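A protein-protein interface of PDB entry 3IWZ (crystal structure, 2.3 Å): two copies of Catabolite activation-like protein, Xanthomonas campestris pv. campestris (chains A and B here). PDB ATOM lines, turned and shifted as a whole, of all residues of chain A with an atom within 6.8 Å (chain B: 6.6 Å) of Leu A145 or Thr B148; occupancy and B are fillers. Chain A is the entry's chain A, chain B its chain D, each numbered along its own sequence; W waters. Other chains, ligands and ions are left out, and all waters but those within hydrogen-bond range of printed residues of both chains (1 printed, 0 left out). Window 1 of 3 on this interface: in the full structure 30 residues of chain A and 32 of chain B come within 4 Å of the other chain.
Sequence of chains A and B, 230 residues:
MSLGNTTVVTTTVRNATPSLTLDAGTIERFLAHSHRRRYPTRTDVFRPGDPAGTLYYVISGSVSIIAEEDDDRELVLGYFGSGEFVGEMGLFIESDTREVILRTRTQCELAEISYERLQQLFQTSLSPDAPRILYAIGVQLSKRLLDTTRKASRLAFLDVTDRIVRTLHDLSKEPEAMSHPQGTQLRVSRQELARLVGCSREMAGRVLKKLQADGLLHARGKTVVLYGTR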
ATOM      1  N   LEU A  77       9.433  14.466  11.299  1.00  0.00           N
ATOM      2  CA  LEU A  77       8.088  14.907  10.970  1.00  0.00           C
ATOM      3  C   LEU A  77       7.004  14.279  11.846  1.00  0.00           C
ATOM      4  O   LEU A  77       5.948  14.876  12.043  1.00  0.00           O
ATOM      5  CB  LEU A  77       7.805  14.593   9.503  1.00  0.00           C
ATOM      6  CG  LEU A  77       8.923  15.027   8.558  1.00  0.00           C
ATOM      7  CD1 LEU A  77       8.662  14.473   7.180  1.00  0.00           C
ATOM      8  CD2 LEU A  77       9.020  16.547   8.528  1.00  0.00           C
ATOM      9  N   GLN A 140      -5.071   9.508   7.417  1.00  0.00           N
ATOM     10  CA  GLN A 140      -3.706   9.650   7.897  1.00  0.00           C
ATOM     11  C   GLN A 140      -2.960  10.760   7.172  1.00  0.00           C
ATOM     12  O   GLN A 140      -2.230  11.531   7.783  1.00  0.00           O
ATOM     13  CB  GLN A 140      -2.987   8.305   7.769  1.00  0.00           C
ATOM     14  CG  GLN A 140      -3.908   7.155   8.127  1.00  0.00           C
ATOM     15  CD  GLN A 140      -3.203   5.849   8.431  1.00  0.00           C
ATOM     16  OE1 GLN A 140      -2.188   5.507   7.825  1.00  0.00           O
ATOM     17  NE2 GLN A 140      -3.764   5.093   9.364  1.00  0.00           N
ATOM     18  N   LEU A 141      -3.162  10.852   5.865  1.00  0.00           N
ATOM     19  CA  LEU A 141      -2.518  11.893   5.086  1.00  0.00           C
ATOM     20  C   LEU A 141      -2.996  13.246   5.626  1.00  0.00           C
ATOM     21  O   LEU A 141      -2.203  14.170   5.777  1.00  0.00           O
ATOM     22  CB  LEU A 141      -2.868  11.738   3.600  1.00  0.00           C
ATOM     23  CG  LEU A 141      -2.186  10.582   2.850  1.00  0.00           C
ATOM     24  CD1 LEU A 141      -2.582  10.593   1.371  1.00  0.00           C
ATOM     25  CD2 LEU A 141      -0.677  10.707   2.981  1.00  0.00           C
ATOM     26  N   SER A 142      -4.292  13.347   5.918  1.00  0.00           N
ATOM     27  CA  SER A 142      -4.874  14.580   6.452  1.00  0.00           C
ATOM     28  C   SER A 142      -4.268  14.930   7.799  1.00  0.00           C
ATOM     29  O   SER A 142      -3.912  16.073   8.044  1.00  0.00           O
ATOM     30  CB  SER A 142      -6.390  14.448   6.609  1.00  0.00           C
ATOM     31  OG  SER A 142      -7.035  14.395   5.348  1.00  0.00           O
ATOM     32  N   LYS A 143      -4.161  13.943   8.682  1.00  0.00           N
ATOM     33  CA  LYS A 143      -3.559  14.202   9.982  1.00  0.00           C
ATOM     34  C   LYS A 143      -2.123  14.692   9.772  1.00  0.00           C
ATOM     35  O   LYS A 143      -1.695  15.686  10.361  1.00  0.00           O
ATOM     36  CB  LYS A 143      -3.532  12.936  10.844  1.00  0.00           C
ATOM     37  CG  LYS A 143      -4.858  12.534  11.473  1.00  0.00           C
ATOM     38  CD  LYS A 143      -4.659  11.280  12.325  1.00  0.00           C
ATOM     39  CE  LYS A 143      -5.980  10.680  12.778  1.00  0.00           C
ATOM     40  NZ  LYS A 143      -6.777  11.616  13.601  1.00  0.00           N
ATOM     41  N   ARG A 144      -1.389  13.985   8.928  1.00  0.00           N
ATOM     42  CA  ARG A 144      -0.004  14.331   8.654  1.00  0.00           C
ATOM     43  C   ARG A 144       0.136  15.718   8.040  1.00  0.00           C
ATOM     44  O   ARG A 144       1.019  16.487   8.414  1.00  0.00           O
ATOM     45  CB  ARG A 144       0.627  13.267   7.755  1.00  0.00           C
ATOM     46  CG  ARG A 144       1.323  12.177   8.561  1.00  0.00           C
ATOM     47  CD  ARG A 144       0.659  10.802   8.503  1.00  0.00           C
ATOM     48  NE  ARG A 144       1.152   9.997   7.390  1.00  0.00           N
ATOM     49  CZ  ARG A 144       0.985   8.678   7.275  1.00  0.00           C
ATOM     50  NH1 ARG A 144       1.471   8.041   6.216  1.00  0.00           N
ATOM     51  NH2 ARG A 144       0.347   7.988   8.219  1.00  0.00           N
ATOM     52  N   LEU A 145      -0.748  16.047   7.107  1.00  0.00           N
ATOM     53  CA  LEU A 145      -0.685  17.358   6.482  1.00  0.00           C
ATOM     54  C   LEU A 145      -0.926  18.425   7.565  1.00  0.00           C
ATOM     55  O   LEU A 145      -0.248  19.450   7.595  1.00  0.00           O
ATOM     56  CB  LEU A 145      -1.725  17.471   5.362  1.00  0.00           C
ATOM     57  CG  LEU A 145      -1.754  18.787   4.570  1.00  0.00           C
ATOM     58  CD1 LEU A 145      -0.369  19.077   3.950  1.00  0.00           C
ATOM     59  CD2 LEU A 145      -2.804  18.678   3.472  1.00  0.00           C
ATOM     60  N   LEU A 146      -1.870  18.167   8.473  1.00  0.00           N
ATOM     61  CA  LEU A 146      -2.157  19.144   9.531  1.00  0.00           C
ATOM     62  C   LEU A 146      -0.922  19.364  10.383  1.00  0.00           C
ATOM     63  O   LEU A 146      -0.412  20.478  10.468  1.00  0.00           O
ATOM     64  CB  LEU A 146      -3.324  18.668  10.404  1.00  0.00           C
ATOM     65  CG  LEU A 146      -3.979  19.633  11.399  1.00  0.00           C
ATOM     66  CD1 LEU A 146      -4.244  21.008  10.752  1.00  0.00           C
ATOM     67  CD2 LEU A 146      -5.289  18.994  11.880  1.00  0.00           C
ATOM     68  N   ASP A 147      -0.439  18.290  10.995  1.00  0.00           N
ATOM     69  CA  ASP A 147       0.747  18.341  11.844  1.00  0.00           C
ATOM     70  C   ASP A 147       1.939  18.977  11.113  1.00  0.00           C
ATOM     71  O   ASP A 147       2.659  19.801  11.676  1.00  0.00           O
ATOM     72  CB  ASP A 147       1.142  16.930  12.311  1.00  0.00           C
ATOM     73  CG  ASP A 147       0.083  16.274  13.213  1.00  0.00           C
ATOM     74  OD1 ASP A 147      -0.955  16.908  13.505  1.00  0.00           O
ATOM     75  OD2 ASP A 147       0.293  15.108  13.630  1.00  0.00           O
ATOM     76  N   THR A 148       2.149  18.599   9.860  1.00  0.00           N
ATOM     77  CA  THR A 148       3.274  19.160   9.121  1.00  0.00           C
ATOM     78  C   THR A 148       3.036  20.632   8.833  1.00  0.00           C
ATOM     79  O   THR A 148       3.957  21.436   8.883  1.00  0.00           O
ATOM     80  CB  THR A 148       3.513  18.384   7.844  1.00  0.00           C
ATOM     81  OG1 THR A 148       3.667  16.999   8.186  1.00  0.00           O
ATOM     82  CG2 THR A 148       4.784  18.874   7.142  1.00  0.00           C
ATOM     83  N   THR A 149       1.785  20.983   8.562  1.00  0.00           N
ATOM     84  CA  THR A 149       1.414  22.374   8.315  1.00  0.00           C
ATOM     85  C   THR A 149       1.715  23.181   9.581  1.00  0.00           C
ATOM     86  O   THR A 149       2.215  24.304   9.506  1.00  0.00           O
ATOM     87  CB  THR A 149      -0.099  22.487   7.964  1.00  0.00           C
ATOM     88  OG1 THR A 149      -0.303  22.031   6.624  1.00  0.00           O
ATOM     89  CG2 THR A 149      -0.595  23.916   8.105  1.00  0.00           C
ATOM     90  N   ARG A 150       1.426  22.600  10.747  1.00  0.00           N
ATOM     91  CA  ARG A 150       1.696  23.281  12.014  1.00  0.00           C
ATOM     92  C   ARG A 150       3.187  23.313  12.315  1.00  0.00           C
ATOM     93  O   ARG A 150       3.667  24.266  12.921  1.00  0.00           O
ATOM     94  CB  ARG A 150       0.936  22.621  13.176  1.00  0.00           C
ATOM     95  CG  ARG A 150      -0.558  22.894  13.143  1.00  0.00           C
ATOM     96  CD  ARG A 150      -1.323  22.084  14.163  1.00  0.00           C
ATOM     97  NE  ARG A 150      -2.754  22.366  14.089  1.00  0.00           N
ATOM     98  CZ  ARG A 150      -3.697  21.610  14.641  1.00  0.00           C
ATOM     99  NH1 ARG A 150      -3.363  20.520  15.314  1.00  0.00           N
ATOM    100  NH2 ARG A 150      -4.977  21.936  14.513  1.00  0.00           N
ATOM    101  N   LYS A 151       3.927  22.282  11.902  1.00  0.00           N
ATOM    102  CA  LYS A 151       5.367  22.299  12.150  1.00  0.00           C
ATOM    103  C   LYS A 151       5.998  23.394  11.279  1.00  0.00           C
ATOM    104  O   LYS A 151       6.898  24.094  11.725  1.00  0.00           O
ATOM    105  CB  LYS A 151       6.026  20.943  11.851  1.00  0.00           C
ATOM    106  CG  LYS A 151       7.400  20.805  12.525  1.00  0.00           C
ATOM    107  CD  LYS A 151       8.273  19.681  11.963  1.00  0.00           C
ATOM    108  CE  LYS A 151       7.953  18.327  12.596  1.00  0.00           C
ATOM    109  NZ  LYS A 151       8.245  18.289  14.071  1.00  0.00           N
ATOM    110  N   ALA A 152       5.524  23.545  10.040  1.00  0.00           N
ATOM    111  CA  ALA A 152       6.053  24.600   9.158  1.00  0.00           C
ATOM    112  C   ALA A 152       5.811  25.997   9.769  1.00  0.00           C
ATOM    113  O   ALA A 152       6.704  26.841   9.764  1.00  0.00           O
ATOM    114  CB  ALA A 152       5.399  24.526   7.799  1.00  0.00           C
ATOM    115  N   LEU B  77       0.995  28.058   2.110  1.00  0.00           N
ATOM    116  CA  LEU B  77       1.417  26.665   2.030  1.00  0.00           C
ATOM    117  C   LEU B  77       1.335  26.186   0.595  1.00  0.00           C
ATOM    118  O   LEU B  77       1.860  25.124   0.261  1.00  0.00           O
ATOM    119  CB  LEU B  77       0.542  25.770   2.906  1.00  0.00           C
ATOM    120  CG  LEU B  77       0.317  26.226   4.343  1.00  0.00           C
ATOM    121  CD1 LEU B  77      -0.429  25.141   5.087  1.00  0.00           C
ATOM    122  CD2 LEU B  77       1.630  26.506   5.018  1.00  0.00           C
ATOM    123  N   GLU B  88     -10.902  20.232   2.390  1.00  0.00           N
ATOM    124  CA  GLU B  88     -11.282  18.839   2.531  1.00  0.00           C
ATOM    125  C   GLU B  88     -10.986  18.187   3.870  1.00  0.00           C
ATOM    126  O   GLU B  88     -11.474  17.093   4.130  1.00  0.00           O
ATOM    127  CB  GLU B  88     -10.623  18.007   1.430  1.00  0.00           C
ATOM    128  CG  GLU B  88      -9.150  17.692   1.662  1.00  0.00           C
ATOM    129  CD  GLU B  88      -8.302  18.926   1.947  1.00  0.00           C
ATOM    130  OE1 GLU B  88      -8.580  20.028   1.395  1.00  0.00           O
ATOM    131  OE2 GLU B  88      -7.342  18.781   2.723  1.00  0.00           O
ATOM    132  N   GLN B 140      -4.000  14.521  -4.218  1.00  0.00           N
ATOM    133  CA  GLN B 140      -3.809  15.914  -3.854  1.00  0.00           C
ATOM    134  C   GLN B 140      -3.261  16.077  -2.450  1.00  0.00           C
ATOM    135  O   GLN B 140      -2.428  16.944  -2.212  1.00  0.00           O
ATOM    136  CB  GLN B 140      -5.116  16.701  -4.045  1.00  0.00           C
ATOM    137  CG  GLN B 140      -5.556  16.727  -5.509  1.00  0.00           C
ATOM    138  CD  GLN B 140      -6.836  17.519  -5.767  1.00  0.00           C
ATOM    139  OE1 GLN B 140      -7.369  17.505  -6.881  1.00  0.00           O
ATOM    140  NE2 GLN B 140      -7.326  18.212  -4.750  1.00  0.00           N
ATOM    141  N   LEU B 141      -3.720  15.242  -1.523  1.00  0.00           N
ATOM    142  CA  LEU B 141      -3.221  15.308  -0.160  1.00  0.00           C
ATOM    143  C   LEU B 141      -1.740  14.939  -0.180  1.00  0.00           C
ATOM    144  O   LEU B 141      -0.931  15.571   0.492  1.00  0.00           O
ATOM    145  CB  LEU B 141      -4.007  14.358   0.760  1.00  0.00           C
ATOM    146  CG  LEU B 141      -5.408  14.835   1.211  1.00  0.00           C
ATOM    147  CD1 LEU B 141      -6.128  13.745   1.998  1.00  0.00           C
ATOM    148  CD2 LEU B 141      -5.270  16.089   2.070  1.00  0.00           C
ATOM    149  N   LYS B 143       0.498  15.339  -2.598  1.00  0.00           N
ATOM    150  CA  LYS B 143       1.364  16.377  -3.164  1.00  0.00           C
ATOM    151  C   LYS B 143       1.607  17.504  -2.167  1.00  0.00           C
ATOM    152  O   LYS B 143       2.720  18.014  -2.051  1.00  0.00           O
ATOM    153  CB  LYS B 143       0.766  16.950  -4.454  1.00  0.00           C
ATOM    154  CG  LYS B 143       0.768  15.983  -5.617  1.00  0.00           C
ATOM    155  CD  LYS B 143      -0.002  16.542  -6.811  1.00  0.00           C
ATOM    156  CE  LYS B 143      -1.480  16.717  -6.467  1.00  0.00           C
ATOM    157  NZ  LYS B 143      -2.253  17.224  -7.635  1.00  0.00           N
ATOM    158  N   ARG B 144       0.561  17.884  -1.444  1.00  0.00           N
ATOM    159  CA  ARG B 144       0.664  18.960  -0.455  1.00  0.00           C
ATOM    160  C   ARG B 144       1.527  18.554   0.722  1.00  0.00           C
ATOM    161  O   ARG B 144       2.276  19.371   1.263  1.00  0.00           O
ATOM    162  CB  ARG B 144      -0.723  19.360   0.038  1.00  0.00           C
ATOM    163  CG  ARG B 144      -1.590  19.955  -1.057  1.00  0.00           C
ATOM    164  CD  ARG B 144      -3.048  20.060  -0.642  1.00  0.00           C
ATOM    165  NE  ARG B 144      -3.911  19.914  -1.813  1.00  0.00           N
ATOM    166  CZ  ARG B 144      -5.231  20.066  -1.816  1.00  0.00           C
ATOM    167  NH1 ARG B 144      -5.899  19.901  -2.951  1.00  0.00           N
ATOM    168  NH2 ARG B 144      -5.882  20.389  -0.699  1.00  0.00           N
ATOM    169  N   LEU B 145       1.410  17.289   1.116  1.00  0.00           N
ATOM    170  CA  LEU B 145       2.197  16.760   2.218  1.00  0.00           C
ATOM    171  C   LEU B 145       3.663  16.831   1.811  1.00  0.00           C
ATOM    172  O   LEU B 145       4.509  17.308   2.573  1.00  0.00           O
ATOM    173  CB  LEU B 145       1.821  15.291   2.516  1.00  0.00           C
ATOM    174  CG  LEU B 145       2.667  14.620   3.614  1.00  0.00           C
ATOM    175  CD1 LEU B 145       2.668  15.518   4.850  1.00  0.00           C
ATOM    176  CD2 LEU B 145       2.118  13.206   3.965  1.00  0.00           C
ATOM    177  N   LEU B 146       3.960  16.353   0.606  1.00  0.00           N
ATOM    178  CA  LEU B 146       5.327  16.362   0.116  1.00  0.00           C
ATOM    179  C   LEU B 146       5.826  17.810   0.057  1.00  0.00           C
ATOM    180  O   LEU B 146       6.919  18.111   0.532  1.00  0.00           O
ATOM    181  CB  LEU B 146       5.403  15.697  -1.272  1.00  0.00           C
ATOM    182  CG  LEU B 146       6.730  15.773  -2.041  1.00  0.00           C
ATOM    183  CD1 LEU B 146       7.840  15.092  -1.247  1.00  0.00           C
ATOM    184  CD2 LEU B 146       6.565  15.114  -3.405  1.00  0.00           C
ATOM    185  N   ASP B 147       5.003  18.703  -0.496  1.00  0.00           N
ATOM    186  CA  ASP B 147       5.372  20.119  -0.602  1.00  0.00           C
ATOM    187  C   ASP B 147       5.567  20.801   0.755  1.00  0.00           C
ATOM    188  O   ASP B 147       6.518  21.567   0.937  1.00  0.00           O
ATOM    189  CB  ASP B 147       4.322  20.909  -1.399  1.00  0.00           C
ATOM    190  CG  ASP B 147       4.368  20.606  -2.884  1.00  0.00           C
ATOM    191  OD1 ASP B 147       5.387  20.046  -3.338  1.00  0.00           O
ATOM    192  OD2 ASP B 147       3.389  20.938  -3.596  1.00  0.00           O
ATOM    193  N   THR B 148       4.674  20.526   1.705  1.00  0.00           N
ATOM    194  CA  THR B 148       4.778  21.135   3.032  1.00  0.00           C
ATOM    195  C   THR B 148       5.944  20.528   3.793  1.00  0.00           C
ATOM    196  O   THR B 148       6.647  21.218   4.535  1.00  0.00           O
ATOM    197  CB  THR B 148       3.486  20.937   3.840  1.00  0.00           C
ATOM    198  OG1 THR B 148       2.381  21.237   3.001  1.00  0.00           O
ATOM    199  CG2 THR B 148       3.452  21.872   5.071  1.00  0.00           C
ATOM    200  N   THR B 149       6.155  19.228   3.610  1.00  0.00           N
ATOM    201  CA  THR B 149       7.276  18.571   4.275  1.00  0.00           C
ATOM    202  C   THR B 149       8.558  19.270   3.835  1.00  0.00           C
ATOM    203  O   THR B 149       9.462  19.523   4.646  1.00  0.00           O
ATOM    204  CB  THR B 149       7.369  17.086   3.895  1.00  0.00           C
ATOM    205  OG1 THR B 149       6.205  16.404   4.366  1.00  0.00           O
ATOM    206  CG2 THR B 149       8.622  16.453   4.493  1.00  0.00           C
ATOM    207  N   ARG B 150       8.627  19.597   2.546  1.00  0.00           N
ATOM    208  CA  ARG B 150       9.811  20.269   2.019  1.00  0.00           C
ATOM    209  C   ARG B 150       9.948  21.672   2.579  1.00  0.00           C
ATOM    210  O   ARG B 150      11.058  22.124   2.867  1.00  0.00           O
ATOM    211  CB  ARG B 150       9.769  20.330   0.487  1.00  0.00           C
ATOM    212  CG  ARG B 150      10.083  19.011  -0.186  1.00  0.00           C
ATOM    213  CD  ARG B 150       9.624  18.972  -1.640  1.00  0.00           C
ATOM    214  NE  ARG B 150      10.097  17.744  -2.276  1.00  0.00           N
ATOM    215  CZ  ARG B 150       9.770  17.355  -3.505  1.00  0.00           C
ATOM    216  NH1 ARG B 150       8.958  18.094  -4.257  1.00  0.00           N
ATOM    217  NH2 ARG B 150      10.260  16.220  -3.985  1.00  0.00           N
ATOM    218  N   LYS B 151       8.820  22.355   2.750  1.00  0.00           N
ATOM    219  CA  LYS B 151       8.832  23.716   3.274  1.00  0.00           C
ATOM    220  C   LYS B 151       9.365  23.729   4.700  1.00  0.00           C
ATOM    221  O   LYS B 151      10.213  24.544   5.053  1.00  0.00           O
ATOM    222  CB  LYS B 151       7.421  24.307   3.246  1.00  0.00           C
ATOM    223  CG  LYS B 151       7.401  25.806   3.073  1.00  0.00           C
ATOM    224  CD  LYS B 151       5.988  26.331   3.076  1.00  0.00           C
ATOM    225  CE  LYS B 151       5.942  27.816   2.778  1.00  0.00           C
ATOM    226  NZ  LYS B 151       5.924  28.104   1.313  1.00  0.00           N
ATOM    227  N   ALA B 152       8.852  22.828   5.525  1.00  0.00           N
ATOM    228  CA  ALA B 152       9.295  22.746   6.904  1.00  0.00           C
ATOM    229  C   ALA B 152      10.803  22.505   6.926  1.00  0.00           C
ATOM    230  O   ALA B 152      11.528  23.103   7.715  1.00  0.00           O
ATOM    231  CB  ALA B 152       8.570  21.609   7.620  1.00  0.00           C
ATOM    232  N   SER B 153      11.268  21.622   6.053  1.00  0.00           N
ATOM    233  CA  SER B 153      12.690  21.316   5.990  1.00  0.00           C
ATOM    234  C   SER B 153      13.470  22.595   5.681  1.00  0.00           C
ATOM    235  O   SER B 153      14.496  22.880   6.307  1.00  0.00           O
ATOM    236  CB  SER B 153      12.941  20.255   4.921  1.00  0.00           C
ATOM    237  OG  SER B 153      14.277  19.804   4.938  1.00  0.00           O
HETATM  238  O   HOH W   1      -6.986  17.256   4.822  1.00  0.00           O
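Water W1 lies within hydrogen-bond range of the side-chain carboxylate (OE2) of Glu B88 and the side-chain hydroxyl (OG) of Ser A142.
Leu A141 touches Leu B145, and with the chains exchanged Leu A145 touches Leu B141.
Leu B145 touches its own counterpart, Leu A145.
Leu A145 touches Thr B148, and with the chains exchanged Thr A148 touches Leu B145.
Thr A148 touches Thr B149, and with the chains exchanged Thr A149 touches Thr B148.
Of the 12 pairs that touch across the chains among the printed residues, 10 have their exchanged pair printed and touching as well.
Leu A145 touches four residues of chain B.
Thr B148 touches just these residues of chain A: Leu A145 (3.6 Å), Thr A148 (3.9 Å) and Thr A149 (3.9 Å).
Printed residues of chain A within 4 Å of Leu B77: Thr A149 (3.3 Å).
Of the printed residues of chain A, Thr B149 touches Leu A77 and Thr A148.
Of the printed residues of chain A, Leu B145 touches Leu A141 (3.9 Å), Leu A145 (3.8 Å) and Thr A148 (3.8 Å).
Of the printed residues of chain B, Ser A142 touches Leu B141.
Of the printed residues of chain A, Leu B141 touches Ser A142 and Leu A145.
The nearest residue of chain A that does not touch Thr B148 is Ala A152 (4.3 Å).
The nearest printed residue of chain A that does not touch Leu B145 is Arg A144 (4.04 Å).
The backbone carbonyl oxygen (O) of Arg A144 sits at hydrogen-bond distance from the side-chain hydroxyl (OG1) of Thr A148 (2.7 Å).
The side-chain hydroxyl (OG1) of Thr A149 is in hydrogen-bond range of the backbone carbonyl oxygen (O) of Leu A145 (2.8 Å).
OE1 of Glu B88 lies within salt-bridge range of NH2 of Arg B144, at 3.4 Å.
The side-chain amide nitrogen (NE2) of Gln B140 sits close to the guanidinium group (NH1) of Arg B144.
O of Arg B144 lies within hydrogen-bond range of OG1 of Thr B148 (2.6 Å).
The backbone carbonyl oxygen of Leu B145 is in hydrogen-bond range of the side-chain hydroxyl of Thr B149 (2.6 Å).
CG2 of Thr B149 touches CD1 of Leu A77, at 3.3 Å.
Leu A141 touches Leu B145 (CD2 to CD2, 3.9 Å).
Leu B141 touches Ser A142.
Leu A145 touches Leu B141.
Arg B144 touches Leu A145.
OG1 of Thr B148 touches CD1 of Leu A145 (3.6 Å).
OG1 of Thr A148 touches CD1 of Leu B145, 3.8 Å away.
Thr A148 touches Thr B148 (O to CG2, 3.9 Å).
N of Thr B149 touches CG2 of Thr A148, 3.8 Å away.
Thr B148 touches Thr A149.
Of the 15 printed residues of chain B, 6 touch a printed residue of chain A.
Printed residues of chain B that touch a printed residue of chain A: Leu B77, Leu B141, Arg B144, Leu B145, Thr B148 and Thr B149.
Printed residues of chain A that touch a printed residue of chain B: Leu A77, Leu A141, Ser A142, Leu A145, Thr A148 and Thr A149.
Along chain A the printed residues that touch a printed residue of chain B span positions 77 to 149.
Among the printed residues, no Asp or Glu carboxylate lies within 4 Å of a Lys or Arg side-chain nitrogen of the other chain.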
